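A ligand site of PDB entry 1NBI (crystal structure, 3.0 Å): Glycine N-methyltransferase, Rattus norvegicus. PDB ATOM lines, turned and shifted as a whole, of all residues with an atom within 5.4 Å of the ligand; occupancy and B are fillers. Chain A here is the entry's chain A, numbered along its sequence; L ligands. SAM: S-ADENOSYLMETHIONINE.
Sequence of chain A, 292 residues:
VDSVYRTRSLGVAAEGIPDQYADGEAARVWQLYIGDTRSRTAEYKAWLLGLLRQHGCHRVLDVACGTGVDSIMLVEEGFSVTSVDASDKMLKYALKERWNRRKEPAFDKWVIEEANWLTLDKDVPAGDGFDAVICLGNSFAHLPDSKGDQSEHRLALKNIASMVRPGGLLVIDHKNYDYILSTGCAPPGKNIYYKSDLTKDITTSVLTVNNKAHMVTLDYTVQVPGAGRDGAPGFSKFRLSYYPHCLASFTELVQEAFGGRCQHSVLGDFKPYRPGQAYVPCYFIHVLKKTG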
ATOM      1  N   ASP A  19      31.290 -11.311  24.821  1.00  0.00           N
ATOM      2  CA  ASP A  19      30.456 -12.114  23.932  1.00  0.00           C
ATOM      3  C   ASP A  19      29.302 -11.254  23.416  1.00  0.00           C
ATOM      4  O   ASP A  19      28.328 -11.032  24.134  1.00  0.00           O
ATOM      5  CB  ASP A  19      29.900 -13.322  24.709  1.00  0.00           C
ATOM      6  CG  ASP A  19      28.991 -14.184  23.867  1.00  0.00           C
ATOM      7  OD1 ASP A  19      28.280 -15.032  24.448  1.00  0.00           O
ATOM      8  OD2 ASP A  19      28.984 -14.020  22.625  1.00  0.00           O
ATOM      9  N   TYR A  21      27.081 -11.994  21.816  1.00  0.00           N
ATOM     10  CA  TYR A  21      25.881 -12.831  21.798  1.00  0.00           C
ATOM     11  C   TYR A  21      25.396 -13.141  23.214  1.00  0.00           C
ATOM     12  O   TYR A  21      24.580 -14.025  23.424  1.00  0.00           O
ATOM     13  CB  TYR A  21      26.176 -14.140  21.036  1.00  0.00           C
ATOM     14  CG  TYR A  21      26.378 -13.944  19.550  1.00  0.00           C
ATOM     15  CD1 TYR A  21      27.527 -13.330  19.062  1.00  0.00           C
ATOM     16  CD2 TYR A  21      25.372 -14.282  18.648  1.00  0.00           C
ATOM     17  CE1 TYR A  21      27.661 -13.038  17.696  1.00  0.00           C
ATOM     18  CE2 TYR A  21      25.498 -13.999  17.289  1.00  0.00           C
ATOM     19  CZ  TYR A  21      26.640 -13.366  16.815  1.00  0.00           C
ATOM     20  OH  TYR A  21      26.735 -13.008  15.483  1.00  0.00           O
ATOM     21  N   TRP A  30      18.184 -15.605  15.218  1.00  0.00           N
ATOM     22  CA  TRP A  30      19.112 -16.117  14.207  1.00  0.00           C
ATOM     23  C   TRP A  30      18.419 -17.018  13.186  1.00  0.00           C
ATOM     24  O   TRP A  30      18.716 -16.982  11.983  1.00  0.00           O
ATOM     25  CB  TRP A  30      20.234 -16.909  14.883  1.00  0.00           C
ATOM     26  CG  TRP A  30      21.535 -16.747  14.211  1.00  0.00           C
ATOM     27  CD1 TRP A  30      22.160 -17.661  13.425  1.00  0.00           C
ATOM     28  CD2 TRP A  30      22.327 -15.564  14.172  1.00  0.00           C
ATOM     29  NE1 TRP A  30      23.305 -17.124  12.895  1.00  0.00           N
ATOM     30  CE2 TRP A  30      23.432 -15.828  13.336  1.00  0.00           C
ATOM     31  CE3 TRP A  30      22.220 -14.293  14.761  1.00  0.00           C
ATOM     32  CZ2 TRP A  30      24.433 -14.870  13.077  1.00  0.00           C
ATOM     33  CZ3 TRP A  30      23.207 -13.334  14.500  1.00  0.00           C
ATOM     34  CH2 TRP A  30      24.301 -13.634  13.664  1.00  0.00           C
ATOM     35  N   ILE A  34      18.971 -15.681   9.715  1.00  0.00           N
ATOM     36  CA  ILE A  34      19.609 -16.465   8.674  1.00  0.00           C
ATOM     37  C   ILE A  34      18.719 -16.465   7.430  1.00  0.00           C
ATOM     38  O   ILE A  34      19.184 -16.322   6.300  1.00  0.00           O
ATOM     39  CB  ILE A  34      19.832 -17.915   9.171  1.00  0.00           C
ATOM     40  CG1 ILE A  34      21.096 -17.961  10.037  1.00  0.00           C
ATOM     41  CG2 ILE A  34      19.952 -18.887   7.985  1.00  0.00           C
ATOM     42  CD1 ILE A  34      21.465 -19.335  10.513  1.00  0.00           C
ATOM     43  N   ARG A  40      19.813 -20.912   2.056  1.00  0.00           N
ATOM     44  CA  ARG A  40      21.125 -20.436   2.463  1.00  0.00           C
ATOM     45  C   ARG A  40      22.123 -21.560   2.228  1.00  0.00           C
ATOM     46  O   ARG A  40      23.204 -21.340   1.666  1.00  0.00           O
ATOM     47  CB  ARG A  40      21.092 -20.043   3.934  1.00  0.00           C
ATOM     48  CG  ARG A  40      22.031 -20.809   4.801  1.00  0.00           C
ATOM     49  CD  ARG A  40      22.906 -19.873   5.574  1.00  0.00           C
ATOM     50  NE  ARG A  40      24.248 -20.411   5.733  1.00  0.00           N
ATOM     51  CZ  ARG A  40      25.053 -20.048   6.728  1.00  0.00           C
ATOM     52  NH1 ARG A  40      24.636 -19.157   7.621  1.00  0.00           N
ATOM     53  NH2 ARG A  40      26.253 -20.581   6.827  1.00  0.00           N
ATOM     54  N   VAL A  63      34.718 -24.330  14.137  1.00  0.00           N
ATOM     55  CA  VAL A  63      35.066 -23.314  15.151  1.00  0.00           C
ATOM     56  C   VAL A  63      34.095 -22.186  15.339  1.00  0.00           C
ATOM     57  O   VAL A  63      34.269 -21.372  16.253  1.00  0.00           O
ATOM     58  CB  VAL A  63      36.429 -22.666  14.880  1.00  0.00           C
ATOM     59  CG1 VAL A  63      37.516 -23.681  14.969  1.00  0.00           C
ATOM     60  CG2 VAL A  63      36.444 -22.012  13.512  1.00  0.00           C
ATOM     61  N   ALA A  64      33.094 -22.099  14.469  1.00  0.00           N
ATOM     62  CA  ALA A  64      32.086 -21.048  14.600  1.00  0.00           C
ATOM     63  C   ALA A  64      30.724 -21.698  14.536  1.00  0.00           C
ATOM     64  O   ALA A  64      29.815 -21.199  13.853  1.00  0.00           O
ATOM     65  CB  ALA A  64      32.239 -20.019  13.488  1.00  0.00           C
ATOM     66  N   CYS A  65      30.579 -22.830  15.224  1.00  0.00           N
ATOM     67  CA  CYS A  65      29.328 -23.582  15.231  1.00  0.00           C
ATOM     68  C   CYS A  65      28.053 -22.764  15.293  1.00  0.00           C
ATOM     69  O   CYS A  65      27.073 -23.087  14.618  1.00  0.00           O
ATOM     70  CB  CYS A  65      29.294 -24.592  16.376  1.00  0.00           C
ATOM     71  SG  CYS A  65      27.645 -25.332  16.497  1.00  0.00           S
ATOM     72  N   GLY A  66      28.060 -21.723  16.119  1.00  0.00           N
ATOM     73  CA  GLY A  66      26.874 -20.889  16.229  1.00  0.00           C
ATOM     74  C   GLY A  66      25.710 -21.780  16.608  1.00  0.00           C
ATOM     75  O   GLY A  66      25.837 -22.602  17.512  1.00  0.00           O
ATOM     76  N   THR A  67      24.573 -21.612  15.929  1.00  0.00           N
ATOM     77  CA  THR A  67      23.410 -22.449  16.218  1.00  0.00           C
ATOM     78  C   THR A  67      23.636 -23.807  15.570  1.00  0.00           C
ATOM     79  O   THR A  67      22.837 -24.723  15.733  1.00  0.00           O
ATOM     80  CB  THR A  67      22.120 -21.857  15.642  1.00  0.00           C
ATOM     81  OG1 THR A  67      22.370 -21.352  14.329  1.00  0.00           O
ATOM     82  CG2 THR A  67      21.605 -20.754  16.516  1.00  0.00           C
ATOM     83  N   VAL A  69      24.189 -24.392  12.051  1.00  0.00           N
ATOM     84  CA  VAL A  69      23.614 -24.547  10.726  1.00  0.00           C
ATOM     85  C   VAL A  69      24.443 -25.435   9.798  1.00  0.00           C
ATOM     86  O   VAL A  69      23.900 -26.300   9.133  1.00  0.00           O
ATOM     87  CB  VAL A  69      23.367 -23.172  10.059  1.00  0.00           C
ATOM     88  CG1 VAL A  69      24.679 -22.540   9.599  1.00  0.00           C
ATOM     89  CG2 VAL A  69      22.429 -23.357   8.883  1.00  0.00           C
ATOM     90  N   ASP A  70      25.751 -25.216   9.759  1.00  0.00           N
ATOM     91  CA  ASP A  70      26.607 -25.994   8.876  1.00  0.00           C
ATOM     92  C   ASP A  70      27.069 -27.306   9.475  1.00  0.00           C
ATOM     93  O   ASP A  70      27.232 -28.301   8.780  1.00  0.00           O
ATOM     94  CB  ASP A  70      27.812 -25.170   8.463  1.00  0.00           C
ATOM     95  CG  ASP A  70      27.405 -23.907   7.712  1.00  0.00           C
ATOM     96  OD1 ASP A  70      27.727 -22.811   8.210  1.00  0.00           O
ATOM     97  OD2 ASP A  70      26.762 -24.027   6.648  1.00  0.00           O
ATOM     98  N   ASP A  85      32.214 -23.226  19.822  1.00  0.00           N
ATOM     99  CA  ASP A  85      31.819 -21.828  19.662  1.00  0.00           C
ATOM    100  C   ASP A  85      31.931 -21.176  21.036  1.00  0.00           C
ATOM    101  O   ASP A  85      31.832 -21.851  22.052  1.00  0.00           O
ATOM    102  CB  ASP A  85      30.380 -21.742  19.117  1.00  0.00           C
ATOM    103  CG  ASP A  85      29.860 -20.313  19.011  1.00  0.00           C
ATOM    104  OD1 ASP A  85      29.734 -19.789  17.880  1.00  0.00           O
ATOM    105  OD2 ASP A  85      29.584 -19.725  20.082  1.00  0.00           O
ATOM    106  N   ALA A  86      32.138 -19.853  21.045  1.00  0.00           N
ATOM    107  CA  ALA A  86      32.311 -19.102  22.287  1.00  0.00           C
ATOM    108  C   ALA A  86      31.038 -18.757  23.036  1.00  0.00           C
ATOM    109  O   ALA A  86      31.044 -18.681  24.260  1.00  0.00           O
ATOM    110  CB  ALA A  86      33.075 -17.838  21.993  1.00  0.00           C
ATOM    111  N   SER A  87      29.961 -18.491  22.308  1.00  0.00           N
ATOM    112  CA  SER A  87      28.696 -18.135  22.937  1.00  0.00           C
ATOM    113  C   SER A  87      27.842 -19.358  23.239  1.00  0.00           C
ATOM    114  O   SER A  87      27.420 -20.081  22.326  1.00  0.00           O
ATOM    115  CB  SER A  87      27.902 -17.172  22.040  1.00  0.00           C
ATOM    116  OG  SER A  87      26.593 -16.903  22.544  1.00  0.00           O
ATOM    117  N   MET A  90      24.187 -19.176  21.759  1.00  0.00           N
ATOM    118  CA  MET A  90      23.974 -19.721  20.421  1.00  0.00           C
ATOM    119  C   MET A  90      24.076 -21.237  20.476  1.00  0.00           C
ATOM    120  O   MET A  90      23.185 -21.957  20.041  1.00  0.00           O
ATOM    121  CB  MET A  90      25.032 -19.182  19.462  1.00  0.00           C
ATOM    122  CG  MET A  90      25.037 -17.682  19.334  1.00  0.00           C
ATOM    123  SD  MET A  90      24.061 -17.186  17.919  1.00  0.00           S
ATOM    124  CE  MET A  90      25.227 -17.434  16.616  1.00  0.00           C
ATOM    125  N   ALA A 115      34.069 -23.140  23.169  1.00  0.00           N
ATOM    126  CA  ALA A 115      35.483 -22.926  22.883  1.00  0.00           C
ATOM    127  C   ALA A 115      35.705 -21.532  22.318  1.00  0.00           C
ATOM    128  O   ALA A 115      34.819 -20.979  21.673  1.00  0.00           O
ATOM    129  CB  ALA A 115      35.980 -23.973  21.897  1.00  0.00           C
ATOM    130  N   ASN A 116      36.887 -20.971  22.563  1.00  0.00           N
ATOM    131  CA  ASN A 116      37.175 -19.635  22.055  1.00  0.00           C
ATOM    132  C   ASN A 116      38.454 -19.621  21.257  1.00  0.00           C
ATOM    133  O   ASN A 116      39.515 -19.961  21.753  1.00  0.00           O
ATOM    134  CB  ASN A 116      37.308 -18.624  23.193  1.00  0.00           C
ATOM    135  CG  ASN A 116      37.451 -17.174  22.685  1.00  0.00           C
ATOM    136  OD1 ASN A 116      38.169 -16.901  21.710  1.00  0.00           O
ATOM    137  ND2 ASN A 116      36.762 -16.258  23.347  1.00  0.00           N
ATOM    138  N   TRP A 117      38.333 -19.182  20.009  1.00  0.00           N
ATOM    139  CA  TRP A 117      39.468 -19.091  19.107  1.00  0.00           C
ATOM    140  C   TRP A 117      40.738 -18.617  19.822  1.00  0.00           C
ATOM    141  O   TRP A 117      41.797 -19.237  19.689  1.00  0.00           O
ATOM    142  CB  TRP A 117      39.110 -18.139  17.954  1.00  0.00           C
ATOM    143  CG  TRP A 117      37.841 -18.544  17.227  1.00  0.00           C
ATOM    144  CD1 TRP A 117      37.320 -19.807  17.137  1.00  0.00           C
ATOM    145  CD2 TRP A 117      36.944 -17.685  16.517  1.00  0.00           C
ATOM    146  NE1 TRP A 117      36.146 -19.785  16.413  1.00  0.00           N
ATOM    147  CE2 TRP A 117      35.893 -18.495  16.025  1.00  0.00           C
ATOM    148  CE3 TRP A 117      36.915 -16.314  16.256  1.00  0.00           C
ATOM    149  CZ2 TRP A 117      34.829 -17.976  15.283  1.00  0.00           C
ATOM    150  CZ3 TRP A 117      35.850 -15.795  15.514  1.00  0.00           C
ATOM    151  CH2 TRP A 117      34.838 -16.628  15.042  1.00  0.00           C
ATOM    152  N   LEU A 118      40.633 -17.543  20.588  1.00  0.00           N
ATOM    153  CA  LEU A 118      41.773 -17.007  21.301  1.00  0.00           C
ATOM    154  C   LEU A 118      42.515 -18.013  22.179  1.00  0.00           C
ATOM    155  O   LEU A 118      43.746 -17.996  22.253  1.00  0.00           O
ATOM    156  CB  LEU A 118      41.361 -15.829  22.167  1.00  0.00           C
ATOM    157  CG  LEU A 118      41.744 -14.430  21.700  1.00  0.00           C
ATOM    158  CD1 LEU A 118      42.206 -14.411  20.223  1.00  0.00           C
ATOM    159  CD2 LEU A 118      40.531 -13.554  21.901  1.00  0.00           C
ATOM    160  N   LEU A 136      32.953 -20.598   8.802  1.00  0.00           N
ATOM    161  CA  LEU A 136      32.082 -19.834   7.902  1.00  0.00           C
ATOM    162  C   LEU A 136      31.154 -18.766   8.478  1.00  0.00           C
ATOM    163  O   LEU A 136      31.151 -18.508   9.687  1.00  0.00           O
ATOM    164  CB  LEU A 136      31.250 -20.818   7.081  1.00  0.00           C
ATOM    165  CG  LEU A 136      32.118 -21.768   6.257  1.00  0.00           C
ATOM    166  CD1 LEU A 136      31.623 -23.210   6.352  1.00  0.00           C
ATOM    167  CD2 LEU A 136      32.094 -21.285   4.826  1.00  0.00           C
ATOM    168  N   GLY A 137      30.383 -18.131   7.590  1.00  0.00           N
ATOM    169  CA  GLY A 137      29.408 -17.115   7.967  1.00  0.00           C
ATOM    170  C   GLY A 137      29.898 -15.786   8.510  1.00  0.00           C
ATOM    171  O   GLY A 137      29.173 -15.083   9.235  1.00  0.00           O
ATOM    172  N   ASN A 138      31.129 -15.425   8.143  1.00  0.00           N
ATOM    173  CA  ASN A 138      31.768 -14.195   8.607  1.00  0.00           C
ATOM    174  C   ASN A 138      31.855 -14.118  10.125  1.00  0.00           C
ATOM    175  O   ASN A 138      31.454 -13.117  10.725  1.00  0.00           O
ATOM    176  CB  ASN A 138      31.047 -12.946   8.090  1.00  0.00           C
ATOM    177  CG  ASN A 138      31.895 -11.691   8.256  1.00  0.00           C
ATOM    178  OD1 ASN A 138      33.115 -11.704   8.016  1.00  0.00           O
ATOM    179  ND2 ASN A 138      31.257 -10.604   8.689  1.00  0.00           N
ATOM    180  N   SER A 139      32.384 -15.164  10.753  1.00  0.00           N
ATOM    181  CA  SER A 139      32.505 -15.179  12.198  1.00  0.00           C
ATOM    182  C   SER A 139      33.758 -14.468  12.650  1.00  0.00           C
ATOM    183  O   SER A 139      33.684 -13.513  13.410  1.00  0.00           O
ATOM    184  CB  SER A 139      32.501 -16.615  12.699  1.00  0.00           C
ATOM    185  OG  SER A 139      31.295 -17.258  12.334  1.00  0.00           O
ATOM    186  N   HIS A 142      34.265 -11.015  13.779  1.00  0.00           N
ATOM    187  CA  HIS A 142      33.755 -10.651  15.081  1.00  0.00           C
ATOM    188  C   HIS A 142      34.894 -10.341  16.047  1.00  0.00           C
ATOM    189  O   HIS A 142      34.694  -9.575  16.989  1.00  0.00           O
ATOM    190  CB  HIS A 142      32.888 -11.778  15.648  1.00  0.00           C
ATOM    191  CG  HIS A 142      31.496 -11.809  15.088  1.00  0.00           C
ATOM    192  ND1 HIS A 142      30.392 -11.349  15.777  1.00  0.00           N
ATOM    193  CD2 HIS A 142      31.034 -12.302  13.917  1.00  0.00           C
ATOM    194  CE1 HIS A 142      29.308 -11.567  15.043  1.00  0.00           C
ATOM    195  NE2 HIS A 142      29.677 -12.146  13.915  1.00  0.00           N
ATOM    196  N   LEU A 143      36.057 -10.940  15.840  1.00  0.00           N
ATOM    197  CA  LEU A 143      37.205 -10.703  16.724  1.00  0.00           C
ATOM    198  C   LEU A 143      37.738  -9.293  16.521  1.00  0.00           C
ATOM    199  O   LEU A 143      38.211  -8.950  15.437  1.00  0.00           O
ATOM    200  CB  LEU A 143      38.309 -11.730  16.456  1.00  0.00           C
ATOM    201  CG  LEU A 143      39.423 -11.785  17.498  1.00  0.00           C
ATOM    202  CD1 LEU A 143      38.883 -12.225  18.839  1.00  0.00           C
ATOM    203  CD2 LEU A 143      40.477 -12.748  17.041  1.00  0.00           C
ATOM    204  N   TYR A 193      24.933 -16.108   3.228  1.00  0.00           N
ATOM    205  CA  TYR A 193      24.703 -16.550   4.602  1.00  0.00           C
ATOM    206  C   TYR A 193      23.534 -15.969   5.347  1.00  0.00           C
ATOM    207  O   TYR A 193      22.981 -16.630   6.220  1.00  0.00           O
ATOM    208  CB  TYR A 193      25.956 -16.321   5.437  1.00  0.00           C
ATOM    209  CG  TYR A 193      27.165 -17.045   4.899  1.00  0.00           C
ATOM    210  CD1 TYR A 193      28.354 -16.350   4.638  1.00  0.00           C
ATOM    211  CD2 TYR A 193      27.136 -18.419   4.660  1.00  0.00           C
ATOM    212  CE1 TYR A 193      29.485 -17.004   4.161  1.00  0.00           C
ATOM    213  CE2 TYR A 193      28.259 -19.092   4.177  1.00  0.00           C
ATOM    214  CZ  TYR A 193      29.427 -18.377   3.928  1.00  0.00           C
ATOM    215  OH  TYR A 193      30.565 -19.014   3.467  1.00  0.00           O
ATOM    216  N   TYR A 194      23.163 -14.725   5.024  1.00  0.00           N
ATOM    217  CA  TYR A 194      22.056 -14.083   5.721  1.00  0.00           C
ATOM    218  C   TYR A 194      21.071 -13.289   4.845  1.00  0.00           C
ATOM    219  O   TYR A 194      21.380 -12.181   4.383  1.00  0.00           O
ATOM    220  CB  TYR A 194      22.631 -13.190   6.827  1.00  0.00           C
ATOM    221  CG  TYR A 194      23.715 -13.862   7.635  1.00  0.00           C
ATOM    222  CD1 TYR A 194      25.064 -13.590   7.397  1.00  0.00           C
ATOM    223  CD2 TYR A 194      23.398 -14.778   8.649  1.00  0.00           C
ATOM    224  CE1 TYR A 194      26.081 -14.218   8.144  1.00  0.00           C
ATOM    225  CE2 TYR A 194      24.399 -15.407   9.405  1.00  0.00           C
ATOM    226  CZ  TYR A 194      25.738 -15.129   9.146  1.00  0.00           C
ATOM    227  OH  TYR A 194      26.735 -15.745   9.883  1.00  0.00           O
HETATM  228  N   SAM L   1      28.278 -19.506  11.406  1.00  0.00           N
HETATM  229  CA  SAM L   1      26.834 -19.310  11.705  1.00  0.00           C
HETATM  230  C   SAM L   1      26.018 -19.256  10.434  1.00  0.00           C
HETATM  231  O   SAM L   1      26.603 -19.359   9.339  1.00  0.00           O
HETATM  232  OXT SAM L   1      24.748 -19.090  10.613  1.00  0.00           O
HETATM  233  CB  SAM L   1      26.637 -18.004  12.427  1.00  0.00           C
HETATM  234  CG  SAM L   1      27.882 -17.554  13.080  1.00  0.00           C
HETATM  235  SD  SAM L   1      27.805 -15.997  13.980  1.00  0.00           S
HETATM  236  CE  SAM L   1      27.671 -14.753  12.698  1.00  0.00           C
HETATM  237  C5' SAM L   1      29.432 -15.840  14.607  1.00  0.00           C
HETATM  238  C4' SAM L   1      29.786 -16.802  15.715  1.00  0.00           C
HETATM  239  O4' SAM L   1      31.135 -16.525  16.064  1.00  0.00           O
HETATM  240  C3' SAM L   1      29.012 -16.517  17.000  1.00  0.00           C
HETATM  241  O3' SAM L   1      28.223 -17.743  17.164  1.00  0.00           O
HETATM  242  C2' SAM L   1      30.018 -16.437  18.114  1.00  0.00           C
HETATM  243  O2' SAM L   1      29.787 -17.033  19.353  1.00  0.00           O
HETATM  244  C1' SAM L   1      31.302 -16.842  17.392  1.00  0.00           C
HETATM  245  N9  SAM L   1      32.509 -16.233  17.904  1.00  0.00           N
HETATM  246  C8  SAM L   1      32.899 -14.916  17.938  1.00  0.00           C
HETATM  247  N7  SAM L   1      34.088 -14.723  18.472  1.00  0.00           N
HETATM  248  C5  SAM L   1      34.509 -16.010  18.832  1.00  0.00           C
HETATM  249  C6  SAM L   1      35.682 -16.509  19.448  1.00  0.00           C
HETATM  250  N6  SAM L   1      36.703 -15.696  19.832  1.00  0.00           N
HETATM  251  N1  SAM L   1      35.804 -17.873  19.661  1.00  0.00           N
HETATM  252  C2  SAM L   1      34.785 -18.670  19.271  1.00  0.00           C
HETATM  253  N3  SAM L   1      33.623 -18.311  18.681  1.00  0.00           N
HETATM  254  C4  SAM L   1      33.542 -16.954  18.482  1.00  0.00           C
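A sulfur (SD) of the ligand lies close to the side-chain hydroxyl (OH) of Tyr 21 (3.5 Å). Merely in contact with the ligand: Ile 34 (3.3 Å), Val 63 (3.96 Å), Gly 66 (3.5 Å), Val 69 (3.6 Å), Asp 70 (3.8 Å), Met 90 (3.1 Å), Ala 115 (3.3 Å), Gly 137 (3.8 Å), Ser 139 (3.3 Å), His 142 (3.5 Å) and Tyr 194 (3.1 Å). Of the 28 residues printed, 21 come within 4 Å of the ligand.
NH1 of Arg 40 lies within salt-bridge range of O of the ligand (2.6 Å). The side-chain carboxylate (OD1) of Asp 85 is in hydrogen-bond range of an oxygen (O3') of the ligand. OD1 of Asn 116 is in hydrogen-bond range of N6 of the ligand (2.7 Å). The backbone NH (N) of Trp 117 sits at hydrogen-bond distance from a nitrogen (N1) of the ligand (2.9 Å). N of Ala 86 sits at hydrogen-bond distance from N3 of the ligand. An oxygen (OXT) of the ligand sits at hydrogen-bond distance from the indole nitrogen of Trp 30, 3.3 Å away. The backbone NH of Ser 87 sits close to an oxygen (O2') of the ligand. O of Ala 64 is in hydrogen-bond range of N of the ligand, at 3.3 Å. The backbone carbonyl oxygen of Leu 136 sits at hydrogen-bond distance from a nitrogen (N) of the ligand (3.5 Å).
The guanidinium group (NH2) of Arg 40 lies within salt-bridge range of the side-chain carboxylate (OD1) of Asp 70, 3.0 Å away. O of Tyr 193 lies close to NH1 of Arg 40, 3.3 Å away. The side-chain carboxylate (OD2) of Asp 85 sits at hydrogen-bond distance from the backbone NH (N) of Ser 87 (2.6 Å). O of Asp 85 sits at hydrogen-bond distance from N of Ala 115 (2.8 Å). O of Gly 137 is in hydrogen-bond range of OH of Tyr 194, 2.6 Å away. N of Ala 86 lies within hydrogen-bond range of O of Ala 115 (3.0 Å). The side-chain hydroxyl (OH) of Tyr 21 sits close to a ring nitrogen (NE2) of His 142. OD2 of Asp 19 lies close to N of Tyr 21, at 2.9 Å.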
